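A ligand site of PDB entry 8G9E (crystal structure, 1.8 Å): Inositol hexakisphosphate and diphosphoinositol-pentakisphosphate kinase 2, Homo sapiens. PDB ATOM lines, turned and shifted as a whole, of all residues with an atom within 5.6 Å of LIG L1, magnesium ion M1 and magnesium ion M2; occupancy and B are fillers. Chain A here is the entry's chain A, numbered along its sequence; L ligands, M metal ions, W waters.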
ATOM      1  N   ARG A  98      11.518   8.596  34.805  1.00  0.00           N
ATOM      2  CA  ARG A  98      11.953   7.199  34.747  1.00  0.00           C
ATOM      3  C   ARG A  98      12.975   6.893  35.838  1.00  0.00           C
ATOM      4  O   ARG A  98      13.076   5.757  36.299  1.00  0.00           O
ATOM      5  CB  ARG A  98      12.578   6.867  33.394  1.00  0.00           C
ATOM      6  CG  ARG A  98      11.622   6.975  32.220  1.00  0.00           C
ATOM      7  CD  ARG A  98      12.217   6.431  30.947  1.00  0.00           C
ATOM      8  NE  ARG A  98      11.557   6.927  29.739  1.00  0.00           N
ATOM      9  CZ  ARG A  98      10.581   6.286  29.127  1.00  0.00           C
ATOM     10  NH1 ARG A  98      10.191   5.132  29.622  1.00  0.00           N
ATOM     11  NH2 ARG A  98       9.995   6.823  28.072  1.00  0.00           N
ATOM     12  N   TYR A 102      12.468   3.784  38.356  1.00  0.00           N
ATOM     13  CA  TYR A 102      13.471   2.749  38.528  1.00  0.00           C
ATOM     14  C   TYR A 102      13.957   2.616  39.982  1.00  0.00           C
ATOM     15  O   TYR A 102      14.193   1.507  40.472  1.00  0.00           O
ATOM     16  CB  TYR A 102      14.614   2.955  37.526  1.00  0.00           C
ATOM     17  CG  TYR A 102      14.395   2.319  36.173  1.00  0.00           C
ATOM     18  CD1 TYR A 102      13.151   1.863  35.763  1.00  0.00           C
ATOM     19  CD2 TYR A 102      15.467   2.109  35.334  1.00  0.00           C
ATOM     20  CE1 TYR A 102      12.993   1.246  34.533  1.00  0.00           C
ATOM     21  CE2 TYR A 102      15.329   1.480  34.112  1.00  0.00           C
ATOM     22  CZ  TYR A 102      14.085   1.037  33.696  1.00  0.00           C
ATOM     23  OH  TYR A 102      13.904   0.399  32.487  1.00  0.00           O
ATOM     24  N   PRO A 113      16.177  -4.166  34.144  1.00  0.00           N
ATOM     25  CA  PRO A 113      17.430  -4.147  33.412  1.00  0.00           C
ATOM     26  C   PRO A 113      18.494  -3.381  34.188  1.00  0.00           C
ATOM     27  O   PRO A 113      18.202  -2.388  34.849  1.00  0.00           O
ATOM     28  CB  PRO A 113      17.101  -3.393  32.127  1.00  0.00           C
ATOM     29  CG  PRO A 113      15.606  -3.507  31.999  1.00  0.00           C
ATOM     30  CD  PRO A 113      15.068  -3.534  33.405  1.00  0.00           C
ATOM     31  N   VAL A 149      19.894   0.235  25.405  1.00  0.00           N
ATOM     32  CA  VAL A 149      18.720   1.056  25.239  1.00  0.00           C
ATOM     33  C   VAL A 149      18.971   2.408  25.911  1.00  0.00           C
ATOM     34  O   VAL A 149      19.555   2.482  26.983  1.00  0.00           O
ATOM     35  CB  VAL A 149      17.490   0.345  25.854  1.00  0.00           C
ATOM     36  CG1 VAL A 149      16.225   1.151  25.638  1.00  0.00           C
ATOM     37  CG2 VAL A 149      17.313  -1.068  25.320  1.00  0.00           C
ATOM     38  N   LYS A 151      16.853   5.772  27.059  1.00  0.00           N
ATOM     39  CA  LYS A 151      15.520   6.301  27.313  1.00  0.00           C
ATOM     40  C   LYS A 151      15.626   7.728  27.842  1.00  0.00           C
ATOM     41  O   LYS A 151      16.353   7.972  28.780  1.00  0.00           O
ATOM     42  CB  LYS A 151      14.800   5.455  28.345  1.00  0.00           C
ATOM     43  CG  LYS A 151      14.734   3.971  28.026  1.00  0.00           C
ATOM     44  CD  LYS A 151      13.731   3.225  28.884  1.00  0.00           C
ATOM     45  CE  LYS A 151      13.673   1.797  28.436  1.00  0.00           C
ATOM     46  NZ  LYS A 151      12.869   1.019  29.396  1.00  0.00           N
ATOM     47  N   ALA A 155       9.356  10.219  31.374  1.00  0.00           N
ATOM     48  CA  ALA A 155       8.615   9.023  31.034  1.00  0.00           C
ATOM     49  C   ALA A 155       7.538   9.321  29.975  1.00  0.00           C
ATOM     50  O   ALA A 155       7.023   8.423  29.313  1.00  0.00           O
ATOM     51  CB  ALA A 155       8.027   8.414  32.288  1.00  0.00           C
ATOM     52  N   ASP A 157       8.198  11.124  27.350  1.00  0.00           N
ATOM     53  CA  ASP A 157       8.933  11.210  26.089  1.00  0.00           C
ATOM     54  C   ASP A 157       9.224   9.780  25.613  1.00  0.00           C
ATOM     55  O   ASP A 157      10.068   9.085  26.196  1.00  0.00           O
ATOM     56  CB  ASP A 157      10.199  12.069  26.262  1.00  0.00           C
ATOM     57  CG  ASP A 157      11.009  12.261  24.995  1.00  0.00           C
ATOM     58  OD1 ASP A 157      10.790  11.510  24.008  1.00  0.00           O
ATOM     59  OD2 ASP A 157      11.894  13.154  24.999  1.00  0.00           O
ATOM     60  N   HIS A 158       8.551   9.380  24.530  1.00  0.00           N
ATOM     61  CA  HIS A 158       8.570   8.015  24.019  1.00  0.00           C
ATOM     62  C   HIS A 158       9.655   7.805  22.967  1.00  0.00           C
ATOM     63  O   HIS A 158       9.692   6.734  22.349  1.00  0.00           O
ATOM     64  CB  HIS A 158       7.150   7.640  23.528  1.00  0.00           C
ATOM     65  CG  HIS A 158       6.157   7.818  24.645  1.00  0.00           C
ATOM     66  ND1 HIS A 158       6.255   7.072  25.794  1.00  0.00           N
ATOM     67  CD2 HIS A 158       5.153   8.712  24.851  1.00  0.00           C
ATOM     68  CE1 HIS A 158       5.303   7.443  26.644  1.00  0.00           C
ATOM     69  NE2 HIS A 158       4.615   8.443  26.095  1.00  0.00           N
ATOM     70  N   ASN A 159      10.591   8.753  22.826  1.00  0.00           N
ATOM     71  CA  ASN A 159      11.694   8.648  21.878  1.00  0.00           C
ATOM     72  C   ASN A 159      12.824   7.835  22.501  1.00  0.00           C
ATOM     73  O   ASN A 159      13.854   8.346  22.891  1.00  0.00           O
ATOM     74  CB  ASN A 159      12.157  10.038  21.403  1.00  0.00           C
ATOM     75  CG  ASN A 159      11.065  10.741  20.649  1.00  0.00           C
ATOM     76  OD1 ASN A 159      10.669  10.299  19.568  1.00  0.00           O
ATOM     77  ND2 ASN A 159      10.537  11.808  21.230  1.00  0.00           N
ATOM     78  N   VAL A 160      12.594   6.541  22.625  1.00  0.00           N
ATOM     79  CA  VAL A 160      13.529   5.561  23.139  1.00  0.00           C
ATOM     80  C   VAL A 160      14.324   4.987  21.959  1.00  0.00           C
ATOM     81  O   VAL A 160      13.731   4.621  20.931  1.00  0.00           O
ATOM     82  CB  VAL A 160      12.740   4.479  23.873  1.00  0.00           C
ATOM     83  CG1 VAL A 160      13.561   3.246  24.185  1.00  0.00           C
ATOM     84  CG2 VAL A 160      12.068   4.999  25.127  1.00  0.00           C
ATOM     85  N   ILE A 162      17.417   2.282  20.540  1.00  0.00           N
ATOM     86  CA  ILE A 162      18.165   1.046  20.743  1.00  0.00           C
ATOM     87  C   ILE A 162      19.367   1.096  19.812  1.00  0.00           C
ATOM     88  O   ILE A 162      19.221   1.483  18.666  1.00  0.00           O
ATOM     89  CB  ILE A 162      17.273  -0.181  20.532  1.00  0.00           C
ATOM     90  CG1 ILE A 162      16.041  -0.062  21.457  1.00  0.00           C
ATOM     91  CG2 ILE A 162      18.089  -1.441  20.769  1.00  0.00           C
ATOM     92  CD1 ILE A 162      15.055  -1.128  21.333  1.00  0.00           C
ATOM     93  N   LEU A 175      12.380   4.474  18.474  1.00  0.00           N
ATOM     94  CA  LEU A 175      10.989   4.228  18.826  1.00  0.00           C
ATOM     95  C   LEU A 175      10.259   5.568  19.038  1.00  0.00           C
ATOM     96  O   LEU A 175      10.877   6.585  19.329  1.00  0.00           O
ATOM     97  CB  LEU A 175      10.917   3.415  20.110  1.00  0.00           C
ATOM     98  CG  LEU A 175      11.223   1.922  20.010  1.00  0.00           C
ATOM     99  CD1 LEU A 175      12.626   1.661  19.465  1.00  0.00           C
ATOM    100  CD2 LEU A 175      11.056   1.274  21.372  1.00  0.00           C
ATOM    101  N   ARG A 177       5.849   7.101  19.971  1.00  0.00           N
ATOM    102  CA  ARG A 177       4.435   6.846  20.093  1.00  0.00           C
ATOM    103  C   ARG A 177       3.931   6.550  18.674  1.00  0.00           C
ATOM    104  O   ARG A 177       4.227   7.282  17.735  1.00  0.00           O
ATOM    105  CB  ARG A 177       3.764   8.000  20.835  1.00  0.00           C
ATOM    106  CG  ARG A 177       2.248   7.892  20.899  1.00  0.00           C
ATOM    107  CD  ARG A 177       1.664   6.706  21.666  1.00  0.00           C
ATOM    108  NE  ARG A 177       1.779   6.805  23.122  1.00  0.00           N
ATOM    109  CZ  ARG A 177       2.561   6.021  23.879  1.00  0.00           C
ATOM    110  NH1 ARG A 177       3.367   5.137  23.328  1.00  0.00           N
ATOM    111  NH2 ARG A 177       2.535   6.140  25.194  1.00  0.00           N
ATOM    112  N   GLU A 201      20.302   1.397  29.470  1.00  0.00           N
ATOM    113  CA  GLU A 201      20.091   0.111  30.103  1.00  0.00           C
ATOM    114  C   GLU A 201      20.427  -1.051  29.173  1.00  0.00           C
ATOM    115  O   GLU A 201      20.481  -0.916  27.964  1.00  0.00           O
ATOM    116  CB  GLU A 201      18.676   0.048  30.658  1.00  0.00           C
ATOM    117  CG  GLU A 201      17.594   0.136  29.652  1.00  0.00           C
ATOM    118  CD  GLU A 201      16.217   0.205  30.302  1.00  0.00           C
ATOM    119  OE1 GLU A 201      15.379  -0.649  29.986  1.00  0.00           O
ATOM    120  OE2 GLU A 201      16.008   1.104  31.112  1.00  0.00           O
ATOM    121  N   GLU A 202      20.713  -2.183  29.811  1.00  0.00           N
ATOM    122  CA  GLU A 202      21.034  -3.386  29.057  1.00  0.00           C
ATOM    123  C   GLU A 202      19.786  -3.799  28.276  1.00  0.00           C
ATOM    124  O   GLU A 202      18.658  -3.668  28.737  1.00  0.00           O
ATOM    125  CB  GLU A 202      21.605  -4.465  29.979  1.00  0.00           C
ATOM    126  CG  GLU A 202      20.593  -5.050  30.894  1.00  0.00           C
ATOM    127  CD  GLU A 202      21.038  -6.219  31.755  1.00  0.00           C
ATOM    128  OE1 GLU A 202      22.089  -6.845  31.406  1.00  0.00           O
ATOM    129  OE2 GLU A 202      20.347  -6.474  32.812  1.00  0.00           O
ATOM    130  N   PHE A 203      20.025  -4.273  27.045  1.00  0.00           N
ATOM    131  CA  PHE A 203      18.964  -4.771  26.205  1.00  0.00           C
ATOM    132  C   PHE A 203      18.671  -6.216  26.651  1.00  0.00           C
ATOM    133  O   PHE A 203      19.574  -7.079  26.689  1.00  0.00           O
ATOM    134  CB  PHE A 203      19.367  -4.673  24.731  1.00  0.00           C
ATOM    135  CG  PHE A 203      18.338  -5.187  23.761  1.00  0.00           C
ATOM    136  CD1 PHE A 203      17.310  -4.360  23.318  1.00  0.00           C
ATOM    137  CD2 PHE A 203      18.344  -6.523  23.377  1.00  0.00           C
ATOM    138  CE1 PHE A 203      16.347  -4.855  22.439  1.00  0.00           C
ATOM    139  CE2 PHE A 203      17.379  -6.999  22.504  1.00  0.00           C
ATOM    140  CZ  PHE A 203      16.395  -6.168  22.036  1.00  0.00           C
ATOM    141  N   MET A 204      17.408  -6.456  26.970  1.00  0.00           N
ATOM    142  CA  MET A 204      16.990  -7.767  27.447  1.00  0.00           C
ATOM    143  C   MET A 204      16.439  -8.567  26.269  1.00  0.00           C
ATOM    144  O   MET A 204      15.505  -8.127  25.592  1.00  0.00           O
ATOM    145  CB  MET A 204      15.906  -7.649  28.520  1.00  0.00           C
ATOM    146  CG  MET A 204      16.233  -6.648  29.623  1.00  0.00           C
ATOM    147  SD  MET A 204      17.765  -6.996  30.458  1.00  0.00           S
ATOM    148  CE  MET A 204      17.420  -8.603  31.171  1.00  0.00           C
ATOM    149  N   PRO A 205      16.999  -9.753  25.982  1.00  0.00           N
ATOM    150  CA  PRO A 205      16.598 -10.501  24.800  1.00  0.00           C
ATOM    151  C   PRO A 205      15.284 -11.238  25.061  1.00  0.00           C
ATOM    152  O   PRO A 205      15.202 -12.097  25.920  1.00  0.00           O
ATOM    153  CB  PRO A 205      17.804 -11.432  24.619  1.00  0.00           C
ATOM    154  CG  PRO A 205      18.274 -11.703  26.033  1.00  0.00           C
ATOM    155  CD  PRO A 205      18.129 -10.367  26.709  1.00  0.00           C
ATOM    156  N   ASP A 210       6.619  -7.870  23.939  1.00  0.00           N
ATOM    157  CA  ASP A 210       6.492  -7.222  25.228  1.00  0.00           C
ATOM    158  C   ASP A 210       5.258  -7.759  25.926  1.00  0.00           C
ATOM    159  O   ASP A 210       4.252  -7.958  25.255  1.00  0.00           O
ATOM    160  CB  ASP A 210       6.137  -5.741  25.070  1.00  0.00           C
ATOM    161  CG  ASP A 210       7.179  -4.947  24.331  1.00  0.00           C
ATOM    162  OD1 ASP A 210       8.345  -5.427  24.339  1.00  0.00           O
ATOM    163  OD2 ASP A 210       6.793  -3.850  23.762  1.00  0.00           O
ATOM    164  N   LYS A 212       2.429  -6.564  28.455  1.00  0.00           N
ATOM    165  CA  LYS A 212       1.796  -5.374  29.012  1.00  0.00           C
ATOM    166  C   LYS A 212       0.841  -5.862  30.098  1.00  0.00           C
ATOM    167  O   LYS A 212       0.025  -6.773  29.861  1.00  0.00           O
ATOM    168  CB  LYS A 212       1.038  -4.613  27.928  1.00  0.00           C
ATOM    169  CG  LYS A 212       1.769  -4.340  26.615  1.00  0.00           C
ATOM    170  CD  LYS A 212       2.318  -2.990  26.502  1.00  0.00           C
ATOM    171  CE  LYS A 212       1.305  -1.928  26.125  1.00  0.00           C
ATOM    172  NZ  LYS A 212       1.990  -0.614  26.135  1.00  0.00           N
ATOM    173  N   SER A 228       7.240  -6.343  19.902  1.00  0.00           N
ATOM    174  CA  SER A 228       8.150  -5.305  20.391  1.00  0.00           C
ATOM    175  C   SER A 228       8.400  -4.271  19.297  1.00  0.00           C
ATOM    176  O   SER A 228       8.765  -4.642  18.185  1.00  0.00           O
ATOM    177  CB  SER A 228       9.459  -5.879  20.814  1.00  0.00           C
ATOM    178  OG  SER A 228      10.349  -4.815  21.158  1.00  0.00           O
ATOM    179  N   PRO A 229       8.249  -2.950  19.581  1.00  0.00           N
ATOM    180  CA  PRO A 229       8.648  -1.904  18.631  1.00  0.00           C
ATOM    181  C   PRO A 229      10.139  -1.931  18.332  1.00  0.00           C
ATOM    182  O   PRO A 229      10.573  -1.399  17.308  1.00  0.00           O
ATOM    183  CB  PRO A 229       8.299  -0.563  19.313  1.00  0.00           C
ATOM    184  CG  PRO A 229       7.409  -0.899  20.441  1.00  0.00           C
ATOM    185  CD  PRO A 229       7.650  -2.364  20.793  1.00  0.00           C
ATOM    186  N   ALA A 230      10.893  -2.566  19.204  1.00  0.00           N
ATOM    187  CA  ALA A 230      12.355  -2.678  18.989  1.00  0.00           C
ATOM    188  C   ALA A 230      12.645  -3.650  17.831  1.00  0.00           C
ATOM    189  O   ALA A 230      13.792  -3.708  17.411  1.00  0.00           O
ATOM    190  CB  ALA A 230      12.995  -3.154  20.256  1.00  0.00           C
ATOM    191  N   ASP A 273       5.139  -2.682  32.006  1.00  0.00           N
ATOM    192  CA  ASP A 273       5.639  -3.546  30.949  1.00  0.00           C
ATOM    193  C   ASP A 273       6.663  -4.495  31.529  1.00  0.00           C
ATOM    194  O   ASP A 273       7.486  -4.063  32.356  1.00  0.00           O
ATOM    195  CB  ASP A 273       6.202  -2.743  29.772  1.00  0.00           C
ATOM    196  CG  ASP A 273       5.162  -1.810  29.172  1.00  0.00           C
ATOM    197  OD1 ASP A 273       3.964  -2.234  29.027  1.00  0.00           O
ATOM    198  OD2 ASP A 273       5.528  -0.695  28.842  1.00  0.00           O
ATOM    199  N   LEU A 275       9.496  -7.636  30.389  1.00  0.00           N
ATOM    200  CA  LEU A 275      10.290  -8.323  29.382  1.00  0.00           C
ATOM    201  C   LEU A 275      10.600  -9.712  29.910  1.00  0.00           C
ATOM    202  O   LEU A 275      11.210  -9.855  30.971  1.00  0.00           O
ATOM    203  CB  LEU A 275      11.584  -7.514  29.155  1.00  0.00           C
ATOM    204  CG  LEU A 275      11.367  -6.047  28.775  1.00  0.00           C
ATOM    205  CD1 LEU A 275      12.698  -5.326  28.660  1.00  0.00           C
ATOM    206  CD2 LEU A 275      10.570  -5.902  27.485  1.00  0.00           C
ATOM    207  N   CYS A 284      10.288  -2.910  32.706  1.00  0.00           N
ATOM    208  CA  CYS A 284      11.070  -1.871  32.030  1.00  0.00           C
ATOM    209  C   CYS A 284      10.333  -0.521  31.965  1.00  0.00           C
ATOM    210  O   CYS A 284      10.905   0.457  31.486  1.00  0.00           O
ATOM    211  CB  CYS A 284      11.493  -2.289  30.641  1.00  0.00           C
ATOM    212  SG  CYS A 284      10.103  -2.435  29.497  1.00  0.00           S
ATOM    213  N   ASP A 285       9.098  -0.432  32.482  1.00  0.00           N
ATOM    214  CA  ASP A 285       8.285   0.761  32.318  1.00  0.00           C
ATOM    215  C   ASP A 285       7.090   0.616  33.249  1.00  0.00           C
ATOM    216  O   ASP A 285       6.521  -0.475  33.313  1.00  0.00           O
ATOM    217  CB  ASP A 285       7.841   0.865  30.869  1.00  0.00           C
ATOM    218  CG  ASP A 285       7.076   2.106  30.461  1.00  0.00           C
ATOM    219  OD1 ASP A 285       7.260   3.166  31.094  1.00  0.00           O
ATOM    220  OD2 ASP A 285       6.322   1.979  29.454  1.00  0.00           O
ATOM    221  N   VAL A 286       6.808   1.685  34.003  1.00  0.00           N
ATOM    222  CA  VAL A 286       5.588   1.775  34.800  1.00  0.00           C
ATOM    223  C   VAL A 286       4.839   3.011  34.350  1.00  0.00           C
ATOM    224  O   VAL A 286       5.326   4.113  34.536  1.00  0.00           O
ATOM    225  CB  VAL A 286       5.851   1.797  36.313  1.00  0.00           C
ATOM    226  CG1 VAL A 286       4.549   1.910  37.107  1.00  0.00           C
ATOM    227  CG2 VAL A 286       6.669   0.591  36.762  1.00  0.00           C
ATOM    228  N   ASN A 287       3.633   2.791  33.794  1.00  0.00           N
ATOM    229  CA  ASN A 287       2.861   3.869  33.177  1.00  0.00           C
ATOM    230  C   ASN A 287       1.828   4.499  34.109  1.00  0.00           C
ATOM    231  O   ASN A 287       1.397   5.636  33.870  1.00  0.00           O
ATOM    232  CB  ASN A 287       2.238   3.402  31.872  1.00  0.00           C
ATOM    233  CG  ASN A 287       3.324   3.055  30.878  1.00  0.00           C
ATOM    234  OD1 ASN A 287       3.220   2.042  30.166  1.00  0.00           O
ATOM    235  ND2 ASN A 287       4.342   3.906  30.832  1.00  0.00           N
HETATM  236  P1  LIG L   1       4.967   3.314  26.738  1.00  0.00           P
HETATM  237  O1  LIG L   1       4.669   1.869  27.216  1.00  0.00           O
HETATM  238  O2  LIG L   1       4.067   3.677  25.556  1.00  0.00           O
HETATM  239  O3  LIG L   1       4.812   4.276  27.943  1.00  0.00           O
HETATM  240  P2  LIG L   1       7.865   4.124  26.881  1.00  0.00           P
HETATM  241  O4  LIG L   1       8.327   5.331  26.104  1.00  0.00           O
HETATM  242  O5  LIG L   1       7.635   4.323  28.358  1.00  0.00           O
HETATM  243  N1  LIG L   1       6.536   3.468  26.130  1.00  0.00           N
HETATM  244  P3  LIG L   1       9.408   1.626  27.318  1.00  0.00           P
HETATM  245  O6  LIG L   1      10.311   1.692  28.495  1.00  0.00           O
HETATM  246  O7  LIG L   1       8.125   0.882  27.517  1.00  0.00           O
HETATM  247  O8  LIG L   1       9.080   3.070  26.690  1.00  0.00           O
HETATM  248  O9  LIG L   1      10.207   1.038  26.058  1.00  0.00           O
HETATM  249  C1  LIG L   1       9.555   0.854  24.820  1.00  0.00           C
HETATM  250  C2  LIG L   1       9.806  -0.556  24.335  1.00  0.00           C
HETATM  251  O10 LIG L   1      11.218  -0.760  24.091  1.00  0.00           O
HETATM  252  C3  LIG L   1       9.409  -1.681  25.300  1.00  0.00           C
HETATM  253  O11 LIG L   1       8.019  -1.921  25.141  1.00  0.00           O
HETATM  254  C4  LIG L   1      10.279  -2.831  24.769  1.00  0.00           C
HETATM  255  O12 LIG L   1       9.788  -3.417  23.579  1.00  0.00           O
HETATM  256  C5  LIG L   1      11.568  -2.082  24.466  1.00  0.00           C
HETATM  257  N2  LIG L   1      12.487  -1.999  25.597  1.00  0.00           N
HETATM  258  C6  LIG L   1      12.582  -1.024  26.573  1.00  0.00           C
HETATM  259  N3  LIG L   1      13.556  -1.242  27.421  1.00  0.00           N
HETATM  260  C7  LIG L   1      14.133  -2.431  26.964  1.00  0.00           C
HETATM  261  C8  LIG L   1      15.226  -3.178  27.413  1.00  0.00           C
HETATM  262  N4  LIG L   1      15.956  -2.828  28.476  1.00  0.00           N
HETATM  263  N5  LIG L   1      15.541  -4.309  26.727  1.00  0.00           N
HETATM  264  C9  LIG L   1      14.800  -4.650  25.666  1.00  0.00           C
HETATM  265  N6  LIG L   1      13.749  -4.017  25.129  1.00  0.00           N
HETATM  266  C10 LIG L   1      13.493  -2.895  25.830  1.00  0.00           C
HETATM  267  C1  LG2 L   2      -2.301   4.883  22.951  1.00  0.00           C
HETATM  268  C2  LG2 L   2      -2.395   6.199  23.702  1.00  0.00           C
HETATM  269  C3  LG2 L   2      -1.805   5.000  25.816  1.00  0.00           C
HETATM  270  C4  LG2 L   2      -1.720   3.646  25.018  1.00  0.00           C
HETATM  271  C5  LG2 L   2      -1.503   6.187  24.914  1.00  0.00           C
HETATM  272  O1  LG2 L   2      -2.508   4.066  17.119  1.00  0.00           O
HETATM  273  P1  LG2 L   2      -4.003   4.095  17.439  1.00  0.00           P
HETATM  274  O2  LG2 L   2      -4.767   2.814  17.215  1.00  0.00           O
HETATM  275  O3  LG2 L   2      -4.732   5.427  17.272  1.00  0.00           O
HETATM  276  C6  LG2 L   2      -4.002   3.945  19.453  1.00  0.00           C
HETATM  277  F1  LG2 L   2      -3.561   2.746  19.843  1.00  0.00           F
HETATM  278  F2  LG2 L   2      -5.268   4.178  19.974  1.00  0.00           F
HETATM  279  P2  LG2 L   2      -2.803   5.131  20.292  1.00  0.00           P
HETATM  280  O4  LG2 L   2      -1.344   4.663  20.120  1.00  0.00           O
HETATM  281  O5  LG2 L   2      -3.242   6.558  19.921  1.00  0.00           O
HETATM  282  O6  LG2 L   2      -3.244   4.874  21.875  1.00  0.00           O
HETATM  283  O7  LG2 L   2      -1.767   7.092  22.781  1.00  0.00           O
HETATM  284  P3  LG2 L   2      -2.369   8.569  22.331  1.00  0.00           P
HETATM  285  O8  LG2 L   2      -3.889   8.509  22.530  1.00  0.00           O
HETATM  286  O9  LG2 L   2      -1.861   8.765  20.917  1.00  0.00           O
HETATM  287  O10 LG2 L   2      -1.678   9.595  23.300  1.00  0.00           O
HETATM  288  O11 LG2 L   2      -1.723   7.403  25.665  1.00  0.00           O
HETATM  289  P4  LG2 L   2      -0.474   8.389  26.020  1.00  0.00           P
HETATM  290  O12 LG2 L   2       0.453   7.535  26.847  1.00  0.00           O
HETATM  291  O13 LG2 L   2      -1.219   9.563  26.770  1.00  0.00           O
HETATM  292  O14 LG2 L   2       0.066   8.790  24.642  1.00  0.00           O
HETATM  293  O15 LG2 L   2      -3.126   5.141  26.275  1.00  0.00           O
HETATM  294  P5  LG2 L   2      -3.551   4.973  27.850  1.00  0.00           P
HETATM  295  O16 LG2 L   2      -2.656   3.951  28.505  1.00  0.00           O
HETATM  296  O17 LG2 L   2      -4.936   4.534  27.684  1.00  0.00           O
HETATM  297  O18 LG2 L   2      -3.432   6.369  28.445  1.00  0.00           O
HETATM  298  O19 LG2 L   2      -2.310   2.605  25.826  1.00  0.00           O
HETATM  299  P6  LG2 L   2      -1.427   1.320  26.342  1.00  0.00           P
HETATM  300  O20 LG2 L   2      -0.218   2.077  27.038  1.00  0.00           O
HETATM  301  O21 LG2 L   2      -2.246   0.418  27.255  1.00  0.00           O
HETATM  302  O22 LG2 L   2      -1.028   0.557  25.050  1.00  0.00           O
HETATM  303  C7  LG2 L   2      -2.569   3.657  23.791  1.00  0.00           C
HETATM  304  O23 LG2 L   2      -2.226   2.536  22.930  1.00  0.00           O
HETATM  305  P7  LG2 L   2      -3.341   1.241  22.685  1.00  0.00           P
HETATM  306  O24 LG2 L   2      -4.789   1.764  22.578  1.00  0.00           O
HETATM  307  O25 LG2 L   2      -3.004   0.398  23.831  1.00  0.00           O
HETATM  308  O26 LG2 L   2      -2.827   0.699  21.349  1.00  0.00           O
HETATM  309 MG    MG M   1       6.013   4.191  29.599  1.00  0.00          MG
HETATM  310 MG    MG M   2       6.204   0.716  27.793  1.00  0.00          MG
HETATM  311  O   HOH W   1       9.059   4.396  23.446  1.00  0.00           O
HETATM  312  O   HOH W   2       2.954   1.917  23.911  1.00  0.00           O
HETATM  313  O   HOH W   3      10.971   3.263  31.521  1.00  0.00           O
HETATM  314  O   HOH W   4       2.325   5.379  28.385  1.00  0.00           O
HETATM  315  O   HOH W   5       6.107   6.139  30.186  1.00  0.00           O
HETATM  316  O   HOH W   6       6.041  -0.489  26.136  1.00  0.00           O
HETATM  317  O   HOH W   7      12.555  -5.760  23.157  1.00  0.00           O
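The side-chain carboxylate of Asp 210 lies within hydrogen-bond range of an oxygen (O12) of LIG L1 (2.6 Å).
OE1 of Glu 201 is in hydrogen-bond range of N4 of LIG L1.
An oxygen (O4) of LIG L1 lies within hydrogen-bond range of a ring nitrogen (ND1) of His 158 (2.7 Å).
The guanidinium group (NH1) of Arg 177 is in salt-bridge range of an oxygen (O2) of LIG L1, 2.8 Å away.
The side-chain amino group of Lys 151 is in salt-bridge range of an oxygen (O6) of LIG L1 (2.8 Å).
O of Glu 202 lies within hydrogen-bond range of N4 of LIG L1, at 2.8 Å.
O12 of LIG L1 is in hydrogen-bond range of OG of Ser 228 (2.9 Å).
N5 of LIG L1 is in hydrogen-bond range of N of Met 204, 2.9 Å away.
An oxygen (O4) of LIG L1 lies within salt-bridge range of the guanidinium group (NH2) of Arg 98 (3.0 Å).
The side-chain amino group of Lys 212 sits close to an oxygen (O1) of LIG L1 (3.8 Å).
NH2 of Arg 177 is in salt-bridge range of O12 of LG2 L2, 3.0 Å away.
O22 of LG2 L2 lies within salt-bridge range of NZ of Lys 212 (3.4 Å).
O of Asp 273 lies within hydrogen-bond range of N of Cys 284, 3.1 Å away.
NH1 of Arg 98 sits close to OD1 of Asp 285, at 3.8 Å.
OE1 of Glu 201 lies within salt-bridge range of NZ of Lys 151 (3.1 Å).
The side-chain hydroxyl of Tyr 102 is in hydrogen-bond range of the side-chain carboxylate of Glu 201, 2.6 Å away.
The side-chain hydroxyl (OH) of Tyr 102 lies within hydrogen-bond range of the side-chain amino group (NZ) of Lys 151, 3.3 Å away.
The backbone NH (N) of Ala 230 lies close to the side-chain hydroxyl (OG) of Ser 228, at 3.0 Å.
The side-chain hydroxyl (OH) of Tyr 102 is in hydrogen-bond range of the backbone carbonyl oxygen (O) of Cys 284 (3.2 Å).
N of Leu 175 sits at hydrogen-bond distance from O of Val 160 (2.8 Å).
An oxygen (O6) of LIG L1 sits close to the backbone carbonyl oxygen (O) of Cys 284.
Merely in contact with LIG L1: Leu 175, Phe 203, Leu 275, Pro 113, Val 149, Pro 229 and Val 160.
Hydrophobic or aromatic side chains that line LIG L1: Pro 113, Val 149, His 158, Val 160, Leu 175, Phe 203, Met 204, Pro 229 and Leu 275.
21 residues have an atom within 4 Å of LIG L1: Arg 98, Pro 113, Val 149, Lys 151, His 158, Val 160, Leu 175, Arg 177, Glu 201, Glu 202, Phe 203, Met 204, Asp 210, Lys 212, Ser 228, Pro 229, Asp 273, Leu 275, Cys 284, Asp 285 and Asn 287.
Of the 29 residues printed, 2 come within 4 Å of magnesium ion M2.
Magnesium ion M1 is bound by water W5 (2.0 Å), O5 of LIG L1 (2.0 Å), O3 of LIG L1 (2.0 Å), ND2 of Asn 287 (2.1 Å), OD1 of Asp 285 (2.2 Å) and OD2 of Asp 285 (2.2 Å).
Magnesium ion M1 has six donor atoms within binding distance.
Magnesium ion M2 is bound by OD2 of Asp 273 (1.9 Å), O7 of LIG L1 (1.9 Å), O1 of LIG L1 (2.0 Å), water W6 (2.1 Å) and OD2 of Asp 285 (2.1 Å).
Water W2 lies within hydrogen-bond range of an oxygen (O2) of LIG L1 (2.7 Å) and the guanidinium group of Arg 177 (3.3 Å).
Water W4 lies within hydrogen-bond range of O12 of LG2 L2 and NH2 of Arg 177.
Water W7 lies within hydrogen-bond range of a nitrogen (N6) of LIG L1 (2.9 Å) and the side-chain hydroxyl of Ser 228 (3.1 Å).
Water W1 bridges O of His 158 (2.7 Å) and O4 of LIG L1 (2.9 Å).
Water W3 lies within hydrogen-bond range of NH1 of Arg 98 (2.8 Å), O of Cys 284 (2.8 Å) and O6 of LIG L1 (3.5 Å).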
